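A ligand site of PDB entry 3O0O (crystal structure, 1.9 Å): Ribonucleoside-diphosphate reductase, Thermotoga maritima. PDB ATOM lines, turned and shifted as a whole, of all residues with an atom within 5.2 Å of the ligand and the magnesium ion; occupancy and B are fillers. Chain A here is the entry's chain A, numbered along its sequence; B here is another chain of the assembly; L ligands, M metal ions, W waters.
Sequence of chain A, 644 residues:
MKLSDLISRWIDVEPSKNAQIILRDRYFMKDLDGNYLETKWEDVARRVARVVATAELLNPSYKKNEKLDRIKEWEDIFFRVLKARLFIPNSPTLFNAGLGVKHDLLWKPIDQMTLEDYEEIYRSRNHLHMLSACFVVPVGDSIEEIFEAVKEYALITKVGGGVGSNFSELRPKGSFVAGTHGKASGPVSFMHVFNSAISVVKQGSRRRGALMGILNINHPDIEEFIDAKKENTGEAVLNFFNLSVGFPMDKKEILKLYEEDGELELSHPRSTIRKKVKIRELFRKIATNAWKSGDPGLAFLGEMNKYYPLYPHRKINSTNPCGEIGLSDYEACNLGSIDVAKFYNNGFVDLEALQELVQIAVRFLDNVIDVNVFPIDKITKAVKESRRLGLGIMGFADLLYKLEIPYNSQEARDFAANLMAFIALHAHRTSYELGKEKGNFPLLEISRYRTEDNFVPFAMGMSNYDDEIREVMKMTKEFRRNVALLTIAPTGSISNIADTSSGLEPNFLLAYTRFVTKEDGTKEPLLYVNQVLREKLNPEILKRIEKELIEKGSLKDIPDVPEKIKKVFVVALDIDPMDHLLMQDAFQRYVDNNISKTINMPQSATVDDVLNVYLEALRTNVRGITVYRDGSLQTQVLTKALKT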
ATOM      1  N   ASP A 141     -22.017  18.421  31.232  1.00  0.00           N
ATOM      2  CA  ASP A 141     -22.362  17.802  29.952  1.00  0.00           C
ATOM      3  C   ASP A 141     -23.815  18.020  29.494  1.00  0.00           C
ATOM      4  O   ASP A 141     -24.555  17.063  29.254  1.00  0.00           O
ATOM      5  CB  ASP A 141     -22.045  16.301  30.002  1.00  0.00           C
ATOM      6  CG  ASP A 141     -21.908  15.692  28.624  1.00  0.00           C
ATOM      7  OD1 ASP A 141     -21.534  16.424  27.689  1.00  0.00           O
ATOM      8  OD2 ASP A 141     -22.191  14.479  28.481  1.00  0.00           O
ATOM      9  N   SER A 142     -24.224  19.281  29.351  1.00  0.00           N
ATOM     10  CA  SER A 142     -25.554  19.597  28.841  1.00  0.00           C
ATOM     11  C   SER A 142     -25.597  20.992  28.237  1.00  0.00           C
ATOM     12  O   SER A 142     -24.788  21.850  28.618  1.00  0.00           O
ATOM     13  CB  SER A 142     -26.620  19.438  29.943  1.00  0.00           C
ATOM     14  OG  SER A 142     -26.509  20.453  30.934  1.00  0.00           O
ATOM     15  N   ILE A 143     -26.520  21.234  27.307  1.00  0.00           N
ATOM     16  CA  ILE A 143     -26.685  22.564  26.712  1.00  0.00           C
ATOM     17  C   ILE A 143     -26.968  23.545  27.826  1.00  0.00           C
ATOM     18  O   ILE A 143     -26.426  24.636  27.853  1.00  0.00           O
ATOM     19  CB  ILE A 143     -27.835  22.611  25.669  1.00  0.00           C
ATOM     20  CG1 ILE A 143     -27.474  21.750  24.463  1.00  0.00           C
ATOM     21  CG2 ILE A 143     -28.114  24.070  25.216  1.00  0.00           C
ATOM     22  CD1 ILE A 143     -26.225  22.228  23.717  1.00  0.00           C
ATOM     23  N   GLU A 144     -27.828  23.147  28.751  1.00  0.00           N
ATOM     24  CA  GLU A 144     -28.144  24.003  29.885  1.00  0.00           C
ATOM     25  C   GLU A 144     -26.868  24.448  30.619  1.00  0.00           C
ATOM     26  O   GLU A 144     -26.616  25.650  30.722  1.00  0.00           O
ATOM     27  CB  GLU A 144     -29.099  23.299  30.847  1.00  0.00           C
ATOM     28  CG  GLU A 144     -29.135  23.909  32.237  1.00  0.00           C
ATOM     29  CD  GLU A 144     -29.959  25.178  32.296  1.00  0.00           C
ATOM     30  OE1 GLU A 144     -30.787  25.425  31.386  1.00  0.00           O
ATOM     31  OE2 GLU A 144     -29.786  25.939  33.282  1.00  0.00           O
ATOM     32  N   ILE A 146     -23.613  24.184  29.766  1.00  0.00           N
ATOM     33  CA  ILE A 146     -22.648  24.807  28.878  1.00  0.00           C
ATOM     34  C   ILE A 146     -22.891  26.302  28.727  1.00  0.00           C
ATOM     35  O   ILE A 146     -21.956  27.110  28.856  1.00  0.00           O
ATOM     36  CB  ILE A 146     -22.660  24.143  27.479  1.00  0.00           C
ATOM     37  CG1 ILE A 146     -22.112  22.712  27.553  1.00  0.00           C
ATOM     38  CG2 ILE A 146     -21.892  24.981  26.463  1.00  0.00           C
ATOM     39  CD1 ILE A 146     -22.332  21.899  26.276  1.00  0.00           C
ATOM     40  N   LEU A 170     -17.626  17.255  28.797  1.00  0.00           N
ATOM     41  CA  LEU A 170     -18.365  17.335  27.544  1.00  0.00           C
ATOM     42  C   LEU A 170     -18.101  16.095  26.716  1.00  0.00           C
ATOM     43  O   LEU A 170     -16.950  15.765  26.445  1.00  0.00           O
ATOM     44  CB  LEU A 170     -17.958  18.580  26.746  1.00  0.00           C
ATOM     45  CG  LEU A 170     -18.282  19.897  27.436  1.00  0.00           C
ATOM     46  CD1 LEU A 170     -18.173  21.040  26.441  1.00  0.00           C
ATOM     47  CD2 LEU A 170     -19.684  19.834  28.055  1.00  0.00           C
ATOM     48  N   ARG A 171     -19.162  15.408  26.289  1.00  0.00           N
ATOM     49  CA  ARG A 171     -18.946  14.130  25.622  1.00  0.00           C
ATOM     50  C   ARG A 171     -18.345  14.415  24.249  1.00  0.00           C
ATOM     51  O   ARG A 171     -18.574  15.484  23.688  1.00  0.00           O
ATOM     52  CB  ARG A 171     -20.262  13.338  25.518  1.00  0.00           C
ATOM     53  CG  ARG A 171     -21.356  14.049  24.703  1.00  0.00           C
ATOM     54  CD  ARG A 171     -22.708  13.312  24.820  1.00  0.00           C
ATOM     55  NE  ARG A 171     -23.353  13.562  26.109  1.00  0.00           N
ATOM     56  CZ  ARG A 171     -24.625  13.324  26.387  1.00  0.00           C
ATOM     57  NH1 ARG A 171     -25.422  12.796  25.458  1.00  0.00           N
ATOM     58  NH2 ARG A 171     -25.107  13.614  27.586  1.00  0.00           N
ATOM     59  N   PHE A 176     -23.817  10.106  20.899  1.00  0.00           N
ATOM     60  CA  PHE A 176     -25.278  10.133  20.856  1.00  0.00           C
ATOM     61  C   PHE A 176     -25.842  11.201  21.799  1.00  0.00           C
ATOM     62  O   PHE A 176     -25.419  11.355  22.943  1.00  0.00           O
ATOM     63  CB  PHE A 176     -25.836   8.738  21.198  1.00  0.00           C
ATOM     64  CG  PHE A 176     -27.319   8.612  21.007  1.00  0.00           C
ATOM     65  CD1 PHE A 176     -28.145   8.357  22.096  1.00  0.00           C
ATOM     66  CD2 PHE A 176     -27.889   8.739  19.756  1.00  0.00           C
ATOM     67  CE1 PHE A 176     -29.508   8.220  21.928  1.00  0.00           C
ATOM     68  CE2 PHE A 176     -29.264   8.614  19.585  1.00  0.00           C
ATOM     69  CZ  PHE A 176     -30.069   8.356  20.681  1.00  0.00           C
ATOM     70  N   VAL A 177     -26.785  11.975  21.285  1.00  0.00           N
ATOM     71  CA  VAL A 177     -27.576  12.880  22.115  1.00  0.00           C
ATOM     72  C   VAL A 177     -29.033  12.387  22.139  1.00  0.00           C
ATOM     73  O   VAL A 177     -29.749  12.475  21.144  1.00  0.00           O
ATOM     74  CB  VAL A 177     -27.471  14.340  21.617  1.00  0.00           C
ATOM     75  CG1 VAL A 177     -28.309  15.262  22.480  1.00  0.00           C
ATOM     76  CG2 VAL A 177     -26.009  14.788  21.631  1.00  0.00           C
ATOM     77  N   ALA A 178     -29.466  11.846  23.273  1.00  0.00           N
ATOM     78  CA  ALA A 178     -30.791  11.234  23.363  1.00  0.00           C
ATOM     79  C   ALA A 178     -31.938  12.206  23.122  1.00  0.00           C
ATOM     80  O   ALA A 178     -32.971  11.841  22.569  1.00  0.00           O
ATOM     81  CB  ALA A 178     -30.968  10.524  24.694  1.00  0.00           C
ATOM     82  N   GLY A 179     -31.748  13.457  23.541  1.00  0.00           N
ATOM     83  CA  GLY A 179     -32.818  14.440  23.478  1.00  0.00           C
ATOM     84  C   GLY A 179     -33.225  14.876  22.079  1.00  0.00           C
ATOM     85  O   GLY A 179     -34.311  15.424  21.876  1.00  0.00           O
ATOM     86  N   THR A 180     -32.369  14.604  21.100  1.00  0.00           N
ATOM     87  CA  THR A 180     -32.580  15.012  19.717  1.00  0.00           C
ATOM     88  C   THR A 180     -32.327  13.847  18.787  1.00  0.00           C
ATOM     89  O   THR A 180     -32.517  13.964  17.581  1.00  0.00           O
ATOM     90  CB  THR A 180     -31.575  16.086  19.312  1.00  0.00           C
ATOM     91  OG1 THR A 180     -30.255  15.592  19.564  1.00  0.00           O
ATOM     92  CG2 THR A 180     -31.801  17.397  20.074  1.00  0.00           C
ATOM     93  N   LYS A 183     -26.136  14.064  17.117  1.00  0.00           N
ATOM     94  CA  LYS A 183     -24.729  13.880  17.439  1.00  0.00           C
ATOM     95  C   LYS A 183     -24.154  15.107  18.138  1.00  0.00           C
ATOM     96  O   LYS A 183     -24.476  16.241  17.782  1.00  0.00           O
ATOM     97  CB  LYS A 183     -23.938  13.540  16.173  1.00  0.00           C
ATOM     98  CG  LYS A 183     -24.415  12.240  15.531  1.00  0.00           C
ATOM     99  CD  LYS A 183     -23.783  11.990  14.184  1.00  0.00           C
ATOM    100  CE  LYS A 183     -24.234  10.652  13.629  1.00  0.00           C
ATOM    101  NZ  LYS A 183     -23.487  10.278  12.407  1.00  0.00           N
ATOM    102  N   ALA A 184     -23.305  14.869  19.154  1.00  0.00           N
ATOM    103  CA  ALA A 184     -22.740  15.952  19.949  1.00  0.00           C
ATOM    104  C   ALA A 184     -21.672  16.700  19.156  1.00  0.00           C
ATOM    105  O   ALA A 184     -20.974  16.110  18.334  1.00  0.00           O
ATOM    106  CB  ALA A 184     -22.154  15.429  21.269  1.00  0.00           C
ATOM    107  N   SER A 185     -21.549  17.994  19.415  1.00  0.00           N
ATOM    108  CA  SER A 185     -20.536  18.802  18.748  1.00  0.00           C
ATOM    109  C   SER A 185     -19.120  18.556  19.286  1.00  0.00           C
ATOM    110  O   SER A 185     -18.148  18.722  18.559  1.00  0.00           O
ATOM    111  CB  SER A 185     -20.875  20.286  18.890  1.00  0.00           C
ATOM    112  OG  SER A 185     -22.157  20.562  18.387  1.00  0.00           O
ATOM    113  N   GLY A 186     -19.024  18.171  20.557  1.00  0.00           N
ATOM    114  CA  GLY A 186     -17.713  17.948  21.186  1.00  0.00           C
ATOM    115  C   GLY A 186     -17.072  19.168  21.820  1.00  0.00           C
ATOM    116  O   GLY A 186     -17.358  20.297  21.428  1.00  0.00           O
ATOM    117  N   PHE A 190     -17.535  23.503  21.327  1.00  0.00           N
ATOM    118  CA  PHE A 190     -18.083  24.415  22.338  1.00  0.00           C
ATOM    119  C   PHE A 190     -17.082  25.506  22.782  1.00  0.00           C
ATOM    120  O   PHE A 190     -17.466  26.650  22.997  1.00  0.00           O
ATOM    121  CB  PHE A 190     -18.706  23.665  23.520  1.00  0.00           C
ATOM    122  CG  PHE A 190     -20.004  22.960  23.159  1.00  0.00           C
ATOM    123  CD1 PHE A 190     -21.105  23.680  22.718  1.00  0.00           C
ATOM    124  CD2 PHE A 190     -20.111  21.580  23.250  1.00  0.00           C
ATOM    125  CE1 PHE A 190     -22.296  23.037  22.364  1.00  0.00           C
ATOM    126  CE2 PHE A 190     -21.305  20.918  22.899  1.00  0.00           C
ATOM    127  CZ  PHE A 190     -22.391  21.645  22.457  1.00  0.00           C
ATOM    128  N   LEU B 128     -39.317  17.597  26.474  1.00  0.00           N
ATOM    129  CA  LEU B 128     -39.071  17.801  25.045  1.00  0.00           C
ATOM    130  C   LEU B 128     -40.391  17.926  24.242  1.00  0.00           C
ATOM    131  O   LEU B 128     -40.362  17.886  23.014  1.00  0.00           O
ATOM    132  CB  LEU B 128     -38.302  16.622  24.476  1.00  0.00           C
ATOM    133  CG  LEU B 128     -36.946  16.276  25.116  1.00  0.00           C
ATOM    134  CD1 LEU B 128     -36.393  14.990  24.509  1.00  0.00           C
ATOM    135  CD2 LEU B 128     -35.993  17.438  24.917  1.00  0.00           C
ATOM    136  N   LYS B 158     -32.703  23.825  20.796  1.00  0.00           N
ATOM    137  CA  LYS B 158     -32.499  22.412  21.140  1.00  0.00           C
ATOM    138  C   LYS B 158     -33.788  21.599  20.968  1.00  0.00           C
ATOM    139  O   LYS B 158     -33.769  20.525  20.370  1.00  0.00           O
ATOM    140  CB  LYS B 158     -31.908  22.263  22.555  1.00  0.00           C
ATOM    141  CG  LYS B 158     -32.111  20.867  23.150  1.00  0.00           C
ATOM    142  CD  LYS B 158     -31.576  20.761  24.564  1.00  0.00           C
ATOM    143  CE  LYS B 158     -31.798  19.337  25.107  1.00  0.00           C
ATOM    144  NZ  LYS B 158     -31.362  19.243  26.521  1.00  0.00           N
ATOM    145  N   VAL B 200     -23.633  25.290  17.238  1.00  0.00           N
ATOM    146  CA  VAL B 200     -23.267  24.031  17.930  1.00  0.00           C
ATOM    147  C   VAL B 200     -24.481  23.317  18.488  1.00  0.00           C
ATOM    148  O   VAL B 200     -24.344  22.350  19.238  1.00  0.00           O
ATOM    149  CB  VAL B 200     -22.229  24.217  19.071  1.00  0.00           C
ATOM    150  CG1 VAL B 200     -20.881  24.608  18.507  1.00  0.00           C
ATOM    151  CG2 VAL B 200     -22.729  25.256  20.090  1.00  0.00           C
ATOM    152  N   VAL B 201     -25.661  23.778  18.124  1.00  0.00           N
ATOM    153  CA  VAL B 201     -26.884  23.110  18.549  1.00  0.00           C
ATOM    154  C   VAL B 201     -27.643  22.655  17.316  1.00  0.00           C
ATOM    155  O   VAL B 201     -27.754  23.414  16.355  1.00  0.00           O
ATOM    156  CB  VAL B 201     -27.770  24.074  19.361  1.00  0.00           C
ATOM    157  CG1 VAL B 201     -29.035  23.380  19.813  1.00  0.00           C
ATOM    158  CG2 VAL B 201     -27.002  24.660  20.530  1.00  0.00           C
ATOM    159  N   LYS B 202     -28.143  21.420  17.289  1.00  0.00           N
ATOM    160  CA  LYS B 202     -29.065  21.006  16.231  1.00  0.00           C
ATOM    161  C   LYS B 202     -30.331  20.395  16.825  1.00  0.00           C
ATOM    162  O   LYS B 202     -30.447  20.263  18.041  1.00  0.00           O
ATOM    163  CB  LYS B 202     -28.405  20.016  15.263  1.00  0.00           C
ATOM    164  CG  LYS B 202     -27.367  20.638  14.345  1.00  0.00           C
ATOM    165  CD  LYS B 202     -25.974  20.044  14.595  1.00  0.00           C
ATOM    166  CE  LYS B 202     -25.701  18.840  13.702  1.00  0.00           C
ATOM    167  NZ  LYS B 202     -25.297  19.283  12.328  1.00  0.00           N
ATOM    168  N   GLN B 203     -31.299  20.055  15.969  1.00  0.00           N
ATOM    169  CA  GLN B 203     -32.495  19.312  16.409  1.00  0.00           C
ATOM    170  C   GLN B 203     -32.513  17.819  16.016  1.00  0.00           C
ATOM    171  O   GLN B 203     -33.181  17.031  16.680  1.00  0.00           O
ATOM    172  CB  GLN B 203     -33.809  19.987  15.982  1.00  0.00           C
ATOM    173  CG  GLN B 203     -35.021  19.556  16.834  1.00  0.00           C
ATOM    174  CD  GLN B 203     -36.300  19.293  16.018  1.00  0.00           C
ATOM    175  OE1 GLN B 203     -36.290  19.328  14.781  1.00  0.00           O
ATOM    176  NE2 GLN B 203     -37.406  19.037  16.722  1.00  0.00           N
HETATM  177  P1  LIG L   1     -27.929  17.767  26.490  1.00  0.00           P
HETATM  178  O1  LIG L   1     -27.776  17.506  27.959  1.00  0.00           O
HETATM  179  O2  LIG L   1     -28.480  19.178  26.363  1.00  0.00           O
HETATM  180  O3  LIG L   1     -28.739  16.646  25.658  1.00  0.00           O
HETATM  181  P2  LIG L   1     -29.973  15.733  26.193  1.00  0.00           P
HETATM  182  O4  LIG L   1     -31.229  16.130  25.454  1.00  0.00           O
HETATM  183  O5  LIG L   1     -30.250  15.831  27.681  1.00  0.00           O
HETATM  184  O6  LIG L   1     -29.523  14.288  25.715  1.00  0.00           O
HETATM  185  P3  LIG L   1     -28.723  13.302  26.710  1.00  0.00           P
HETATM  186  O7  LIG L   1     -28.061  12.351  25.727  1.00  0.00           O
HETATM  187  O8  LIG L   1     -27.744  14.127  27.500  1.00  0.00           O
HETATM  188  O9  LIG L   1     -29.597  12.611  27.718  1.00  0.00           O
HETATM  189  O10 LIG L   1     -26.527  17.635  25.688  1.00  0.00           O
HETATM  190  C1  LIG L   1     -25.521  16.736  26.126  1.00  0.00           C
HETATM  191  C2  LIG L   1     -24.218  16.924  25.352  1.00  0.00           C
HETATM  192  O11 LIG L   1     -24.468  16.907  23.951  1.00  0.00           O
HETATM  193  C3  LIG L   1     -23.545  18.258  25.672  1.00  0.00           C
HETATM  194  O12 LIG L   1     -22.109  18.124  25.528  1.00  0.00           O
HETATM  195  C4  LIG L   1     -24.077  19.164  24.581  1.00  0.00           C
HETATM  196  C5  LIG L   1     -24.148  18.213  23.395  1.00  0.00           C
HETATM  197  N1  LIG L   1     -25.165  18.653  22.419  1.00  0.00           N
HETATM  198  C6  LIG L   1     -24.747  19.001  21.101  1.00  0.00           C
HETATM  199  O13 LIG L   1     -23.541  18.928  20.818  1.00  0.00           O
HETATM  200  N2  LIG L   1     -25.629  19.401  20.174  1.00  0.00           N
HETATM  201  C7  LIG L   1     -26.935  19.488  20.470  1.00  0.00           C
HETATM  202  O14 LIG L   1     -27.751  19.866  19.604  1.00  0.00           O
HETATM  203  C8  LIG L   1     -27.404  19.139  21.825  1.00  0.00           C
HETATM  204  C9  LIG L   1     -28.857  19.215  22.170  1.00  0.00           C
HETATM  205  C10 LIG L   1     -26.462  18.717  22.763  1.00  0.00           C
HETATM  206 MG    MG M   1     -28.507  15.695  29.107  1.00  0.00          MG
HETATM  207  O   HOH W   1     -26.465  15.469  30.220  1.00  0.00           O
HETATM  208  O   HOH W   2     -28.562  17.449  18.532  1.00  0.00           O
HETATM  209  O   HOH W   3     -24.690  19.315  17.760  1.00  0.00           O
HETATM  210  O   HOH W   4     -29.363  13.691  29.813  1.00  0.00           O
HETATM  211  O   HOH W   5     -32.354  17.115  28.167  1.00  0.00           O
HETATM  212  O   HOH W   6     -20.218  17.660  23.197  1.00  0.00           O
HETATM  213  O   HOH W   7     -27.257   9.959  26.165  1.00  0.00           O
HETATM  214  O   HOH W   8     -29.477  16.687  30.890  1.00  0.00           O
HETATM  215  O   HOH W   9     -29.662  21.051  28.528  1.00  0.00           O
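N of Ser 185 lies within hydrogen-bond range of O13 of the ligand (2.6 Å). O13 of the ligand sits at hydrogen-bond distance from OG of Ser 185 (3.2 Å). The guanidinium group of Arg 171 is in salt-bridge range of an oxygen (O7) of the ligand (2.7 Å). OD1 of Asp 141 lies within hydrogen-bond range of O12 of the ligand (2.8 Å). An oxygen (O14) of the ligand is in hydrogen-bond range of the backbone NH of Lys 202 of chain B (2.8 Å). The backbone NH (N) of Ala 178 is in hydrogen-bond range of an oxygen (O7) of the ligand (2.9 Å). The side-chain amino group (NZ) of Lys 158 of chain B lies within salt-bridge range of an oxygen (O2) of the ligand (2.9 Å). The backbone NH of Ile 143 lies within hydrogen-bond range of an oxygen (O2) of the ligand (3.0 Å). O6 of the ligand is in hydrogen-bond range of N of Gly 179, 3.2 Å away. O of Val 200 of chain B is in hydrogen-bond range of N2 of the ligand (3.4 Å).
O of Val 200 of chain B lies within hydrogen-bond range of OG of Ser 185 (3.0 Å). The guanidinium group (NE) of Arg 171 is in salt-bridge range of the side-chain carboxylate (OD2) of Asp 141. The guanidinium group of Arg 171 is in hydrogen-bond range of the backbone carbonyl oxygen of Phe 176 (2.9 Å).
Ser 142 touches the ligand (CB to O1, 3.0 Å). CD1 of Ile 146 touches C4 of the ligand, 3.7 Å away. Leu 170 touches the ligand (CD2 to O12, 3.9 Å). O of Phe 176 touches O7 of the ligand (3.97 Å). Val 177 touches the ligand. Ala 184 touches the ligand. CZ of Phe 190 touches O13 of the ligand (3.4 Å). CA of Val 201 of chain B touches O14 of the ligand, at 3.5 Å. Hydrophobic or aromatic side chains within 4 Å of the ligand: Ile 143, Ile 146, Leu 170, Val 177, Ala 178, Ala 184, Phe 190 and Val 201 of chain B. Along chain A the residues within 4 Å of the ligand span positions 141 to 190. The nearest printed residue that does not touch the ligand is Thr 180 (4.05 Å).
No residue comes within 4 Å of the magnesium ion.
O5 of the ligand is bound to the magnesium ion, at 2.3 Å. The magnesium ion is bound by water W8, at 2.3 Å. O1 of the ligand is bound to the magnesium ion. The magnesium ion is bound by water W4 (2.3 Å). The magnesium ion is bound by water W1, at 2.3 Å. The magnesium ion is bound by O8 of the ligand (2.4 Å). The magnesium ion has six donor atoms within binding distance.
Water W1 lies within hydrogen-bond range of O of Asp 141 (2.7 Å) and NH2 of Arg 171 (3.5 Å). Water W5 lies within hydrogen-bond range of NZ of Lys 158 of chain B and O4 of the ligand. Water W7 bridges an oxygen (O7) of the ligand (2.6 Å) and the guanidinium group of Arg 171 (3.5 Å). Water W3 lies within hydrogen-bond range of a nitrogen (N2) of the ligand, the side-chain hydroxyl (OG) of Ser 185, the backbone carbonyl oxygen (O) of Lys 183 and the backbone carbonyl oxygen (O) of Val 200 of chain B. Water W2 lies within hydrogen-bond range of OG1 of Thr 180 (2.7 Å), O14 of the ligand (2.8 Å) and O of Lys 202 of chain B (3.4 Å). Water W6 lies within hydrogen-bond range of O of Arg 171 (2.8 Å), N of Gly 186 (2.9 Å) and O12 of the ligand (3.0 Å).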
